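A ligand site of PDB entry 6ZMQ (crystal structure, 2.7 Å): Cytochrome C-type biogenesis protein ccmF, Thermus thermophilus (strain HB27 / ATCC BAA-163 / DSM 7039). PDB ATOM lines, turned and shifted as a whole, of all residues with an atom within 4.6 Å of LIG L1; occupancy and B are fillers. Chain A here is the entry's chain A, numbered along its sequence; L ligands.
CD1 of Leu 228 touches O4 of LIG L1, 3.3 Å away. Trp 231 touches LIG L1 (CZ2 to C25, 3.4 Å). Leu 275 touches LIG L1. Phe 279 touches LIG L1. Leu 366 touches LIG L1 (CD2 to C2, 3.4 Å). Gly 369 touches LIG L1. Phe 373 touches LIG L1 (CE2 to C19, 3.6 Å). Ile 416 touches LIG L1 (O to C18, 3.6 Å). Leu 419 touches LIG L1 (O to C17, 3.3 Å). Met 420 touches LIG L1. CG1 of Val 509 touches C26 of LIG L1, 3.5 Å away. CG2 of Val 513 touches C26 of LIG L1 (3.0 Å). CG2 of Ile 644 touches O4 of LIG L1 (3.4 Å). Hydrophobic or aromatic side chains within 4 Å of LIG L1: Leu 228, Trp 231, Leu 275, His 276, Phe 279, Leu 366, Phe 373, Met 420, Val 509, His 510, Val 513 and Ile 644.
NE2 of His 510 binds FE1 of LIG L1. A ring nitrogen (NE2) of His 276 binds an iron atom (FE1) of LIG L1 (2.3 Å). An oxygen (O3) of LIG L1 lies within salt-bridge range of the guanidinium group (NH1) of Arg 224, 2.5 Å away. An oxygen (O1) of LIG L1 sits at hydrogen-bond distance from the side-chain hydroxyl (OG) of Ser 506, 2.7 Å away. O2 of LIG L1 lies within salt-bridge range of NH2 of Arg 503, at 3.1 Å. An oxygen (O3) of LIG L1 is in salt-bridge range of the guanidinium group (NH1) of Arg 502, 3.4 Å away.
A ring nitrogen (ND1) of His 510 lies within hydrogen-bond range of the backbone carbonyl oxygen (O) of Ser 506, at 3.1 Å. A ring nitrogen (ND1) of His 276 sits at hydrogen-bond distance from the backbone carbonyl oxygen of Thr 272 (3.3 Å). OG of Ser 506 is in hydrogen-bond range of O of Arg 503, at 2.9 Å. The backbone carbonyl oxygen (O) of Arg 502 sits close to the side-chain hydroxyl (OG) of Ser 506 (3.3 Å). The side-chain hydroxyl of Thr 272 is in hydrogen-bond range of the indole nitrogen of Trp 231 (2.7 Å).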
ATOM      1  N   ARG A 224      35.827  14.255  12.381  1.00  0.00           N
ATOM      2  CA  ARG A 224      35.286  13.705  13.635  1.00  0.00           C
ATOM      3  C   ARG A 224      34.227  14.602  14.263  1.00  0.00           C
ATOM      4  O   ARG A 224      33.250  14.089  14.849  1.00  0.00           O
ATOM      5  CB  ARG A 224      36.482  13.462  14.575  1.00  0.00           C
ATOM      6  CG  ARG A 224      36.214  13.285  16.054  1.00  0.00           C
ATOM      7  CD  ARG A 224      36.495  14.554  16.902  1.00  0.00           C
ATOM      8  NE  ARG A 224      36.562  14.330  18.354  1.00  0.00           N
ATOM      9  CZ  ARG A 224      35.578  13.910  19.153  1.00  0.00           C
ATOM     10  NH1 ARG A 224      35.846  13.650  20.426  1.00  0.00           N
ATOM     11  NH2 ARG A 224      34.338  13.739  18.720  1.00  0.00           N
ATOM     12  N   LEU A 228      30.322  13.753  15.454  1.00  0.00           N
ATOM     13  CA  LEU A 228      29.770  13.953  16.799  1.00  0.00           C
ATOM     14  C   LEU A 228      28.589  14.939  16.784  1.00  0.00           C
ATOM     15  O   LEU A 228      27.549  14.657  17.379  1.00  0.00           O
ATOM     16  CB  LEU A 228      30.839  14.455  17.768  1.00  0.00           C
ATOM     17  CG  LEU A 228      30.257  14.834  19.143  1.00  0.00           C
ATOM     18  CD1 LEU A 228      29.697  13.640  19.948  1.00  0.00           C
ATOM     19  CD2 LEU A 228      31.179  15.675  19.968  1.00  0.00           C
ATOM     20  N   TRP A 231      25.513  13.359  15.188  1.00  0.00           N
ATOM     21  CA  TRP A 231      24.876  12.474  16.153  1.00  0.00           C
ATOM     22  C   TRP A 231      24.223  13.235  17.297  1.00  0.00           C
ATOM     23  O   TRP A 231      23.230  12.768  17.858  1.00  0.00           O
ATOM     24  CB  TRP A 231      25.908  11.487  16.693  1.00  0.00           C
ATOM     25  CG  TRP A 231      25.353  10.513  17.667  1.00  0.00           C
ATOM     26  CD1 TRP A 231      24.848   9.283  17.381  1.00  0.00           C
ATOM     27  CD2 TRP A 231      25.249  10.672  19.101  1.00  0.00           C
ATOM     28  NE1 TRP A 231      24.424   8.666  18.524  1.00  0.00           N
ATOM     29  CE2 TRP A 231      24.658   9.499  19.597  1.00  0.00           C
ATOM     30  CE3 TRP A 231      25.580  11.690  19.996  1.00  0.00           C
ATOM     31  CZ2 TRP A 231      24.393   9.308  20.940  1.00  0.00           C
ATOM     32  CZ3 TRP A 231      25.307  11.503  21.340  1.00  0.00           C
ATOM     33  CH2 TRP A 231      24.734  10.313  21.797  1.00  0.00           C
ATOM     34  N   THR A 272      25.334   5.877  16.027  1.00  0.00           N
ATOM     35  CA  THR A 272      25.942   5.644  17.348  1.00  0.00           C
ATOM     36  C   THR A 272      27.004   4.583  17.161  1.00  0.00           C
ATOM     37  O   THR A 272      28.104   4.749  17.652  1.00  0.00           O
ATOM     38  CB  THR A 272      24.954   5.011  18.296  1.00  0.00           C
ATOM     39  OG1 THR A 272      23.985   6.032  18.285  1.00  0.00           O
ATOM     40  CG2 THR A 272      25.494   4.929  19.700  1.00  0.00           C
ATOM     41  N   LEU A 275      29.838   6.194  15.539  1.00  0.00           N
ATOM     42  CA  LEU A 275      30.600   7.104  16.418  1.00  0.00           C
ATOM     43  C   LEU A 275      31.661   6.320  17.188  1.00  0.00           C
ATOM     44  O   LEU A 275      32.801   6.734  17.242  1.00  0.00           O
ATOM     45  CB  LEU A 275      29.548   7.715  17.339  1.00  0.00           C
ATOM     46  CG  LEU A 275      29.941   8.997  18.012  1.00  0.00           C
ATOM     47  CD1 LEU A 275      28.759   9.621  18.660  1.00  0.00           C
ATOM     48  CD2 LEU A 275      30.976   8.717  19.049  1.00  0.00           C
ATOM     49  N   HIS A 276      31.263   5.206  17.772  1.00  0.00           N
ATOM     50  CA  HIS A 276      32.191   4.329  18.506  1.00  0.00           C
ATOM     51  C   HIS A 276      33.253   3.741  17.575  1.00  0.00           C
ATOM     52  O   HIS A 276      34.359   3.698  17.998  1.00  0.00           O
ATOM     53  CB  HIS A 276      31.400   3.284  19.309  1.00  0.00           C
ATOM     54  CG  HIS A 276      30.692   3.832  20.501  1.00  0.00           C
ATOM     55  ND1 HIS A 276      29.910   4.923  20.452  1.00  0.00           N
ATOM     56  CD2 HIS A 276      30.645   3.426  21.761  1.00  0.00           C
ATOM     57  CE1 HIS A 276      29.432   5.171  21.624  1.00  0.00           C
ATOM     58  NE2 HIS A 276      29.874   4.287  22.453  1.00  0.00           N
ATOM     59  N   PHE A 279      35.688   6.473  16.717  1.00  0.00           N
ATOM     60  CA  PHE A 279      36.598   6.702  17.835  1.00  0.00           C
ATOM     61  C   PHE A 279      37.685   5.631  17.884  1.00  0.00           C
ATOM     62  O   PHE A 279      38.817   5.975  18.104  1.00  0.00           O
ATOM     63  CB  PHE A 279      35.793   6.606  19.118  1.00  0.00           C
ATOM     64  CG  PHE A 279      36.680   6.519  20.306  1.00  0.00           C
ATOM     65  CD1 PHE A 279      37.408   7.614  20.708  1.00  0.00           C
ATOM     66  CD2 PHE A 279      36.858   5.333  20.962  1.00  0.00           C
ATOM     67  CE1 PHE A 279      38.270   7.518  21.783  1.00  0.00           C
ATOM     68  CE2 PHE A 279      37.726   5.248  22.032  1.00  0.00           C
ATOM     69  CZ  PHE A 279      38.423   6.345  22.444  1.00  0.00           C
ATOM     70  N   ARG A 362      39.032  -3.509  24.918  1.00  0.00           N
ATOM     71  CA  ARG A 362      38.116  -2.382  24.770  1.00  0.00           C
ATOM     72  C   ARG A 362      37.650  -2.251  23.325  1.00  0.00           C
ATOM     73  O   ARG A 362      36.505  -1.868  23.055  1.00  0.00           O
ATOM     74  CB  ARG A 362      38.791  -1.094  25.284  1.00  0.00           C
ATOM     75  CG  ARG A 362      37.928   0.159  25.202  1.00  0.00           C
ATOM     76  CD  ARG A 362      38.668   1.465  25.510  1.00  0.00           C
ATOM     77  NE  ARG A 362      39.101   1.600  26.903  1.00  0.00           N
ATOM     78  CZ  ARG A 362      40.004   2.476  27.318  1.00  0.00           C
ATOM     79  NH1 ARG A 362      40.573   3.305  26.456  1.00  0.00           N
ATOM     80  NH2 ARG A 362      40.334   2.537  28.599  1.00  0.00           N
ATOM     81  N   ALA A 365      34.957  -4.995  22.980  1.00  0.00           N
ATOM     82  CA  ALA A 365      33.722  -4.540  23.629  1.00  0.00           C
ATOM     83  C   ALA A 365      33.024  -3.470  22.803  1.00  0.00           C
ATOM     84  O   ALA A 365      31.795  -3.515  22.652  1.00  0.00           O
ATOM     85  CB  ALA A 365      34.027  -4.040  25.042  1.00  0.00           C
ATOM     86  N   LEU A 366      33.786  -2.518  22.242  1.00  0.00           N
ATOM     87  CA  LEU A 366      33.163  -1.463  21.434  1.00  0.00           C
ATOM     88  C   LEU A 366      32.638  -2.027  20.115  1.00  0.00           C
ATOM     89  O   LEU A 366      31.587  -1.586  19.624  1.00  0.00           O
ATOM     90  CB  LEU A 366      34.129  -0.308  21.122  1.00  0.00           C
ATOM     91  CG  LEU A 366      34.741   0.725  22.090  1.00  0.00           C
ATOM     92  CD1 LEU A 366      34.956   2.077  21.381  1.00  0.00           C
ATOM     93  CD2 LEU A 366      34.023   0.903  23.396  1.00  0.00           C
ATOM     94  N   GLY A 369      29.520  -3.926  20.872  1.00  0.00           N
ATOM     95  CA  GLY A 369      28.448  -2.970  21.112  1.00  0.00           C
ATOM     96  C   GLY A 369      27.913  -2.343  19.843  1.00  0.00           C
ATOM     97  O   GLY A 369      26.707  -2.159  19.681  1.00  0.00           O
ATOM     98  N   PHE A 373      24.180  -2.493  18.250  1.00  0.00           N
ATOM     99  CA  PHE A 373      23.446  -1.372  17.661  1.00  0.00           C
ATOM    100  C   PHE A 373      22.984  -1.687  16.233  1.00  0.00           C
ATOM    101  O   PHE A 373      21.817  -1.452  15.878  1.00  0.00           O
ATOM    102  CB  PHE A 373      24.323  -0.118  17.658  1.00  0.00           C
ATOM    103  CG  PHE A 373      24.358   0.621  18.976  1.00  0.00           C
ATOM    104  CD1 PHE A 373      23.203   1.185  19.502  1.00  0.00           C
ATOM    105  CD2 PHE A 373      25.550   0.770  19.659  1.00  0.00           C
ATOM    106  CE1 PHE A 373      23.248   1.873  20.700  1.00  0.00           C
ATOM    107  CE2 PHE A 373      25.603   1.450  20.865  1.00  0.00           C
ATOM    108  CZ  PHE A 373      24.448   1.997  21.373  1.00  0.00           C
ATOM    109  N   ILE A 416      23.605  -3.530  25.572  1.00  0.00           N
ATOM    110  CA  ILE A 416      24.400  -2.307  25.389  1.00  0.00           C
ATOM    111  C   ILE A 416      24.608  -1.591  26.727  1.00  0.00           C
ATOM    112  O   ILE A 416      25.666  -0.995  26.952  1.00  0.00           O
ATOM    113  CB  ILE A 416      23.828  -1.369  24.305  1.00  0.00           C
ATOM    114  CG1 ILE A 416      22.470  -0.750  24.671  1.00  0.00           C
ATOM    115  CG2 ILE A 416      23.749  -2.107  22.986  1.00  0.00           C
ATOM    116  CD1 ILE A 416      21.909   0.105  23.563  1.00  0.00           C
ATOM    117  N   LEU A 419      27.505  -3.516  28.213  1.00  0.00           N
ATOM    118  CA  LEU A 419      28.766  -3.364  27.508  1.00  0.00           C
ATOM    119  C   LEU A 419      29.348  -1.968  27.683  1.00  0.00           C
ATOM    120  O   LEU A 419      30.576  -1.802  27.733  1.00  0.00           O
ATOM    121  CB  LEU A 419      28.570  -3.674  26.028  1.00  0.00           C
ATOM    122  CG  LEU A 419      28.736  -5.158  25.708  1.00  0.00           C
ATOM    123  CD1 LEU A 419      27.906  -5.580  24.501  1.00  0.00           C
ATOM    124  CD2 LEU A 419      30.194  -5.452  25.486  1.00  0.00           C
ATOM    125  N   MET A 420      28.474  -0.957  27.792  1.00  0.00           N
ATOM    126  CA  MET A 420      28.860   0.425  28.061  1.00  0.00           C
ATOM    127  C   MET A 420      29.587   0.580  29.389  1.00  0.00           C
ATOM    128  O   MET A 420      30.552   1.342  29.508  1.00  0.00           O
ATOM    129  CB  MET A 420      27.618   1.290  27.982  1.00  0.00           C
ATOM    130  CG  MET A 420      27.711   2.676  28.512  1.00  0.00           C
ATOM    131  SD  MET A 420      26.109   3.488  28.546  1.00  0.00           S
ATOM    132  CE  MET A 420      25.174   2.579  27.311  1.00  0.00           C
ATOM    133  N   GLY A 423      33.122  -1.868  29.006  1.00  0.00           N
ATOM    134  CA  GLY A 423      34.049  -1.623  27.923  1.00  0.00           C
ATOM    135  C   GLY A 423      35.226  -0.695  28.198  1.00  0.00           C
ATOM    136  O   GLY A 423      36.379  -1.090  28.016  1.00  0.00           O
ATOM    137  N   PRO A 424      34.958   0.553  28.620  1.00  0.00           N
ATOM    138  CA  PRO A 424      36.053   1.481  28.945  1.00  0.00           C
ATOM    139  C   PRO A 424      36.923   1.108  30.153  1.00  0.00           C
ATOM    140  O   PRO A 424      37.964   1.742  30.372  1.00  0.00           O
ATOM    141  CB  PRO A 424      35.318   2.807  29.194  1.00  0.00           C
ATOM    142  CG  PRO A 424      33.828   2.409  29.229  1.00  0.00           C
ATOM    143  CD  PRO A 424      33.773   1.320  28.240  1.00  0.00           C
ATOM    144  N   ARG A 502      36.754  14.725  26.495  1.00  0.00           N
ATOM    145  CA  ARG A 502      36.157  13.535  25.885  1.00  0.00           C
ATOM    146  C   ARG A 502      35.728  12.516  26.933  1.00  0.00           C
ATOM    147  O   ARG A 502      34.572  12.074  26.931  1.00  0.00           O
ATOM    148  CB  ARG A 502      37.142  12.901  24.908  1.00  0.00           C
ATOM    149  CG  ARG A 502      37.817  13.825  23.918  1.00  0.00           C
ATOM    150  CD  ARG A 502      38.716  12.995  23.018  1.00  0.00           C
ATOM    151  NE  ARG A 502      37.955  12.167  22.097  1.00  0.00           N
ATOM    152  CZ  ARG A 502      38.471  11.527  21.053  1.00  0.00           C
ATOM    153  NH1 ARG A 502      37.685  10.896  20.194  1.00  0.00           N
ATOM    154  NH2 ARG A 502      39.787  11.574  20.839  1.00  0.00           N
ATOM    155  N   ARG A 503      36.625  12.199  27.872  1.00  0.00           N
ATOM    156  CA  ARG A 503      36.326  11.182  28.883  1.00  0.00           C
ATOM    157  C   ARG A 503      35.248  11.632  29.863  1.00  0.00           C
ATOM    158  O   ARG A 503      34.297  10.891  30.092  1.00  0.00           O
ATOM    159  CB  ARG A 503      37.601  10.797  29.647  1.00  0.00           C
ATOM    160  CG  ARG A 503      38.590   9.869  28.904  1.00  0.00           C
ATOM    161  CD  ARG A 503      38.192   8.390  28.919  1.00  0.00           C
ATOM    162  NE  ARG A 503      39.227   7.508  28.372  1.00  0.00           N
ATOM    163  CZ  ARG A 503      39.520   7.360  27.082  1.00  0.00           C
ATOM    164  NH1 ARG A 503      40.570   6.623  26.717  1.00  0.00           N
ATOM    165  NH2 ARG A 503      38.820   7.995  26.146  1.00  0.00           N
ATOM    166  N   SER A 506      31.899  12.173  28.060  1.00  0.00           N
ATOM    167  CA  SER A 506      31.402  10.855  27.683  1.00  0.00           C
ATOM    168  C   SER A 506      30.837  10.118  28.888  1.00  0.00           C
ATOM    169  O   SER A 506      29.839   9.410  28.748  1.00  0.00           O
ATOM    170  CB  SER A 506      32.518  10.033  27.035  1.00  0.00           C
ATOM    171  OG  SER A 506      33.217   9.276  27.995  1.00  0.00           O
ATOM    172  N   VAL A 509      27.452  11.572  29.594  1.00  0.00           N
ATOM    173  CA  VAL A 509      26.572  11.024  28.538  1.00  0.00           C
ATOM    174  C   VAL A 509      26.279   9.553  28.811  1.00  0.00           C
ATOM    175  O   VAL A 509      25.145   9.138  28.724  1.00  0.00           O
ATOM    176  CB  VAL A 509      27.274  11.189  27.182  1.00  0.00           C
ATOM    177  CG1 VAL A 509      26.739  10.242  26.145  1.00  0.00           C
ATOM    178  CG2 VAL A 509      27.190  12.594  26.689  1.00  0.00           C
ATOM    179  N   HIS A 510      27.284   8.803  29.222  1.00  0.00           N
ATOM    180  CA  HIS A 510      27.048   7.366  29.458  1.00  0.00           C
ATOM    181  C   HIS A 510      26.043   7.198  30.582  1.00  0.00           C
ATOM    182  O   HIS A 510      25.091   6.369  30.403  1.00  0.00           O
ATOM    183  CB  HIS A 510      28.348   6.591  29.677  1.00  0.00           C
ATOM    184  CG  HIS A 510      29.142   6.358  28.449  1.00  0.00           C
ATOM    185  ND1 HIS A 510      30.497   6.427  28.464  1.00  0.00           N
ATOM    186  CD2 HIS A 510      28.783   6.245  27.155  1.00  0.00           C
ATOM    187  CE1 HIS A 510      30.954   6.282  27.258  1.00  0.00           C
ATOM    188  NE2 HIS A 510      29.919   6.140  26.411  1.00  0.00           N
ATOM    189  N   VAL A 513      22.516   7.938  29.530  1.00  0.00           N
ATOM    190  CA  VAL A 513      21.759   6.808  28.938  1.00  0.00           C
ATOM    191  C   VAL A 513      21.388   5.820  30.034  1.00  0.00           C
ATOM    192  O   VAL A 513      20.352   5.257  29.900  1.00  0.00           O
ATOM    193  CB  VAL A 513      22.458   6.065  27.804  1.00  0.00           C
ATOM    194  CG1 VAL A 513      22.088   4.605  27.796  1.00  0.00           C
ATOM    195  CG2 VAL A 513      22.071   6.661  26.496  1.00  0.00           C
ATOM    196  N   MET A 637      22.393  14.434  28.867  1.00  0.00           N
ATOM    197  CA  MET A 637      22.995  14.163  27.560  1.00  0.00           C
ATOM    198  C   MET A 637      23.312  15.445  26.793  1.00  0.00           C
ATOM    199  O   MET A 637      24.346  15.537  26.128  1.00  0.00           O
ATOM    200  CB  MET A 637      22.054  13.282  26.739  1.00  0.00           C
ATOM    201  CG  MET A 637      22.482  11.851  26.595  1.00  0.00           C
ATOM    202  SD  MET A 637      21.247  11.005  25.612  1.00  0.00           S
ATOM    203  CE  MET A 637      20.209  10.379  26.909  1.00  0.00           C
ATOM    204  N   THR A 641      27.240  16.256  25.848  1.00  0.00           N
ATOM    205  CA  THR A 641      27.711  16.332  24.465  1.00  0.00           C
ATOM    206  C   THR A 641      28.143  17.767  24.117  1.00  0.00           C
ATOM    207  O   THR A 641      29.065  17.977  23.313  1.00  0.00           O
ATOM    208  CB  THR A 641      26.622  15.799  23.536  1.00  0.00           C
ATOM    209  OG1 THR A 641      26.394  14.420  23.852  1.00  0.00           O
ATOM    210  CG2 THR A 641      26.979  15.870  22.037  1.00  0.00           C
ATOM    211  N   ILE A 644      31.732  17.846  25.477  1.00  0.00           N
ATOM    212  CA  ILE A 644      32.752  17.334  24.544  1.00  0.00           C
ATOM    213  C   ILE A 644      33.241  18.451  23.617  1.00  0.00           C
ATOM    214  O   ILE A 644      34.441  18.567  23.318  1.00  0.00           O
ATOM    215  CB  ILE A 644      32.213  16.122  23.741  1.00  0.00           C
ATOM    216  CG1 ILE A 644      31.519  15.112  24.672  1.00  0.00           C
ATOM    217  CG2 ILE A 644      33.354  15.468  22.938  1.00  0.00           C
ATOM    218  CD1 ILE A 644      32.435  14.087  25.310  1.00  0.00           C
HETATM  219  C1  LIG L   1      32.375   7.867  23.896  1.00  0.00           C
HETATM  220  C2  LIG L   1      32.087   3.108  25.020  1.00  0.00           C
HETATM  221  C3  LIG L   1      27.252   3.204  24.146  1.00  0.00           C
HETATM  222  C4  LIG L   1      27.569   8.031  23.520  1.00  0.00           C
HETATM  223  C5  LIG L   1      32.673   6.565  24.268  1.00  0.00           C
HETATM  224  C6  LIG L   1      33.985   6.109  24.536  1.00  0.00           C
HETATM  225  C7  LIG L   1      33.917   4.781  24.837  1.00  0.00           C
HETATM  226  C8  LIG L   1      32.568   4.383  24.770  1.00  0.00           C
HETATM  227  C9  LIG L   1      35.065   3.880  25.201  1.00  0.00           C
HETATM  228  C10 LIG L   1      35.262   6.937  24.490  1.00  0.00           C
HETATM  229  C11 LIG L   1      35.428   7.793  25.765  1.00  0.00           C
HETATM  230  C12 LIG L   1      35.587   6.932  26.994  1.00  0.00           C
HETATM  231  O1  LIG L   1      34.749   7.003  27.922  1.00  0.00           O
HETATM  232  O2  LIG L   1      36.555   6.149  27.085  1.00  0.00           O
HETATM  233  C13 LIG L   1      30.729   2.754  24.841  1.00  0.00           C
HETATM  234  C14 LIG L   1      30.274   1.421  24.883  1.00  0.00           C
HETATM  235  C15 LIG L   1      28.933   1.433  24.642  1.00  0.00           C
HETATM  236  C16 LIG L   1      28.559   2.826  24.414  1.00  0.00           C
HETATM  237  C17 LIG L   1      31.098   0.201  25.162  1.00  0.00           C
HETATM  238  C18 LIG L   1      28.010   0.285  24.579  1.00  0.00           C
HETATM  239  C19 LIG L   1      27.735  -0.216  23.211  1.00  0.00           C
HETATM  240  C20 LIG L   1      26.918   4.539  23.993  1.00  0.00           C
HETATM  241  C21 LIG L   1      25.618   5.044  23.987  1.00  0.00           C
HETATM  242  C22 LIG L   1      25.743   6.396  23.807  1.00  0.00           C
HETATM  243  C23 LIG L   1      27.112   6.733  23.708  1.00  0.00           C
HETATM  244  C24 LIG L   1      24.321   4.296  24.131  1.00  0.00           C
HETATM  245  C25 LIG L   1      24.628   7.333  23.732  1.00  0.00           C
HETATM  246  C26 LIG L   1      24.229   8.105  24.935  1.00  0.00           C
HETATM  247  C27 LIG L   1      28.920   8.415  23.506  1.00  0.00           C
HETATM  248  C28 LIG L   1      29.406   9.766  23.190  1.00  0.00           C
HETATM  249  C29 LIG L   1      30.759   9.735  23.292  1.00  0.00           C
HETATM  250  C30 LIG L   1      31.084   8.347  23.683  1.00  0.00           C
HETATM  251  C31 LIG L   1      28.567  10.964  22.814  1.00  0.00           C
HETATM  252  C32 LIG L   1      31.722  10.884  23.053  1.00  0.00           C
HETATM  253  C33 LIG L   1      32.423  10.685  21.705  1.00  0.00           C
HETATM  254  C34 LIG L   1      33.315  11.822  21.283  1.00  0.00           C
HETATM  255  O3  LIG L   1      34.563  11.733  21.346  1.00  0.00           O
HETATM  256  O4  LIG L   1      32.806  12.870  20.837  1.00  0.00           O
HETATM  257  N1  LIG L   1      31.827   5.479  24.409  1.00  0.00           N
HETATM  258  N2  LIG L   1      29.687   3.549  24.545  1.00  0.00           N
HETATM  259  N3  LIG L   1      27.807   5.574  23.855  1.00  0.00           N
HETATM  260  N4  LIG L   1      29.950   7.645  23.790  1.00  0.00           N
HETATM  261 FE1  LIG L   1      29.811   5.615  24.300  1.00  0.00          FE
HETATM  262  C1  LG2 L   2       8.137  -5.893  30.546  1.00  0.00           C
HETATM  263  C2  LG2 L   2      10.370 -11.320  27.049  1.00  0.00           C
HETATM  264  C3  LG2 L   2       9.725 -11.512  28.418  1.00  0.00           C
HETATM  265  O1  LG2 L   2       8.340  -4.661  29.927  1.00  0.00           O
HETATM  266  C4  LG2 L   2       9.296  -7.938  31.391  1.00  0.00           C
HETATM  267  C5  LG2 L   2       9.487  -6.576  30.718  1.00  0.00           C
HETATM  268  O2  LG2 L   2      10.332  -5.782  31.498  1.00  0.00           O
HETATM  269  C6  LG2 L   2      11.454  -5.326  30.796  1.00  0.00           C
HETATM  270  O3  LG2 L   2      11.550  -4.174  30.519  1.00  0.00           O
HETATM  271  C7  LG2 L   2      12.543  -6.323  30.377  1.00  0.00           C
HETATM  272  C8  LG2 L   2      13.871  -6.020  31.066  1.00  0.00           C
HETATM  273  C9  LG2 L   2      14.592  -7.346  31.328  1.00  0.00           C
HETATM  274  C10 LG2 L   2      15.169  -7.890  30.023  1.00  0.00           C
HETATM  275  C11 LG2 L   2      15.973  -9.166  30.288  1.00  0.00           C
HETATM  276  C12 LG2 L   2      17.474  -8.933  30.139  1.00  0.00           C
HETATM  277  C13 LG2 L   2      18.213 -10.165  30.692  1.00  0.00           C
HETATM  278  C14 LG2 L   2      19.726 -10.073  30.506  1.00  0.00           C
HETATM  279  C15 LG2 L   2      20.392 -11.137  31.389  1.00  0.00           C
HETATM  280  C16 LG2 L   2      21.829 -10.790  31.786  1.00  0.00           C
HETATM  281  C17 LG2 L   2      22.230 -11.621  33.017  1.00  0.00           C
HETATM  282  C18 LG2 L   2      23.381 -12.574  32.695  1.00  0.00           C
HETATM  283  C19 LG2 L   2      23.863 -13.284  33.970  1.00  0.00           C
HETATM  284  C20 LG2 L   2      25.274 -13.833  33.767  1.00  0.00           C
HETATM  285  C21 LG2 L   2      25.913 -14.153  35.129  1.00  0.00           C
HETATM  286  C22 LG2 L   2      27.382 -13.749  35.084  1.00  0.00           C
HETATM  287  C23 LG2 L   2      28.249 -15.009  35.011  1.00  0.00           C
HETATM  288  C24 LG2 L   2      29.588 -14.663  34.381  1.00  0.00           C
HETATM  289  C25 LG2 L   2      29.382 -14.368  32.898  1.00  0.00           C
HETATM  290  C26 LG2 L   2       7.431  -4.361  28.904  1.00  0.00           C
HETATM  291  C27 LG2 L   2       7.862  -3.492  27.716  1.00  0.00           C
HETATM  292  O4  LG2 L   2       6.329  -4.776  28.938  1.00  0.00           O
HETATM  293  C28 LG2 L   2       9.388  -3.324  27.705  1.00  0.00           C
HETATM  294  C29 LG2 L   2       9.796  -2.511  26.481  1.00  0.00           C
HETATM  295  C30 LG2 L   2      11.256  -2.807  26.149  1.00  0.00           C
HETATM  296  C31 LG2 L   2      12.154  -2.178  27.198  1.00  0.00           C
HETATM  297  C32 LG2 L   2      13.194  -1.305  26.507  1.00  0.00           C
HETATM  298  C33 LG2 L   2      14.494  -1.298  27.308  1.00  0.00           C
HETATM  299  C34 LG2 L   2      15.512  -0.483  26.527  1.00  0.00           C
HETATM  300  C35 LG2 L   2      16.554   0.105  27.478  1.00  0.00           C
HETATM  301  C36 LG2 L   2      17.231   1.300  26.821  1.00  0.00           C
HETATM  302  C37 LG2 L   2      18.732   1.159  27.057  1.00  0.00           C
HETATM  303  C38 LG2 L   2      19.452   2.412  26.546  1.00  0.00           C
HETATM  304  C39 LG2 L   2      19.373   2.435  25.029  1.00  0.00           C
HETATM  305  C40 LG2 L   2      20.389   3.437  24.469  1.00  0.00           C
HETATM  306  P1  LG2 L   2       8.432 -10.164  30.251  1.00  0.00           P
HETATM  307  O5  LG2 L   2       9.549 -10.264  29.051  1.00  0.00           O
HETATM  308  O6  LG2 L   2       8.857 -11.017  31.419  1.00  0.00           O
HETATM  309  O7  LG2 L   2       7.108 -10.677  29.744  1.00  0.00           O
HETATM  310  O8  LG2 L   2       8.247  -8.599  30.746  1.00  0.00           O
HETATM  311  N1  LG2 L   2      10.811 -12.594  26.515  1.00  0.00           N
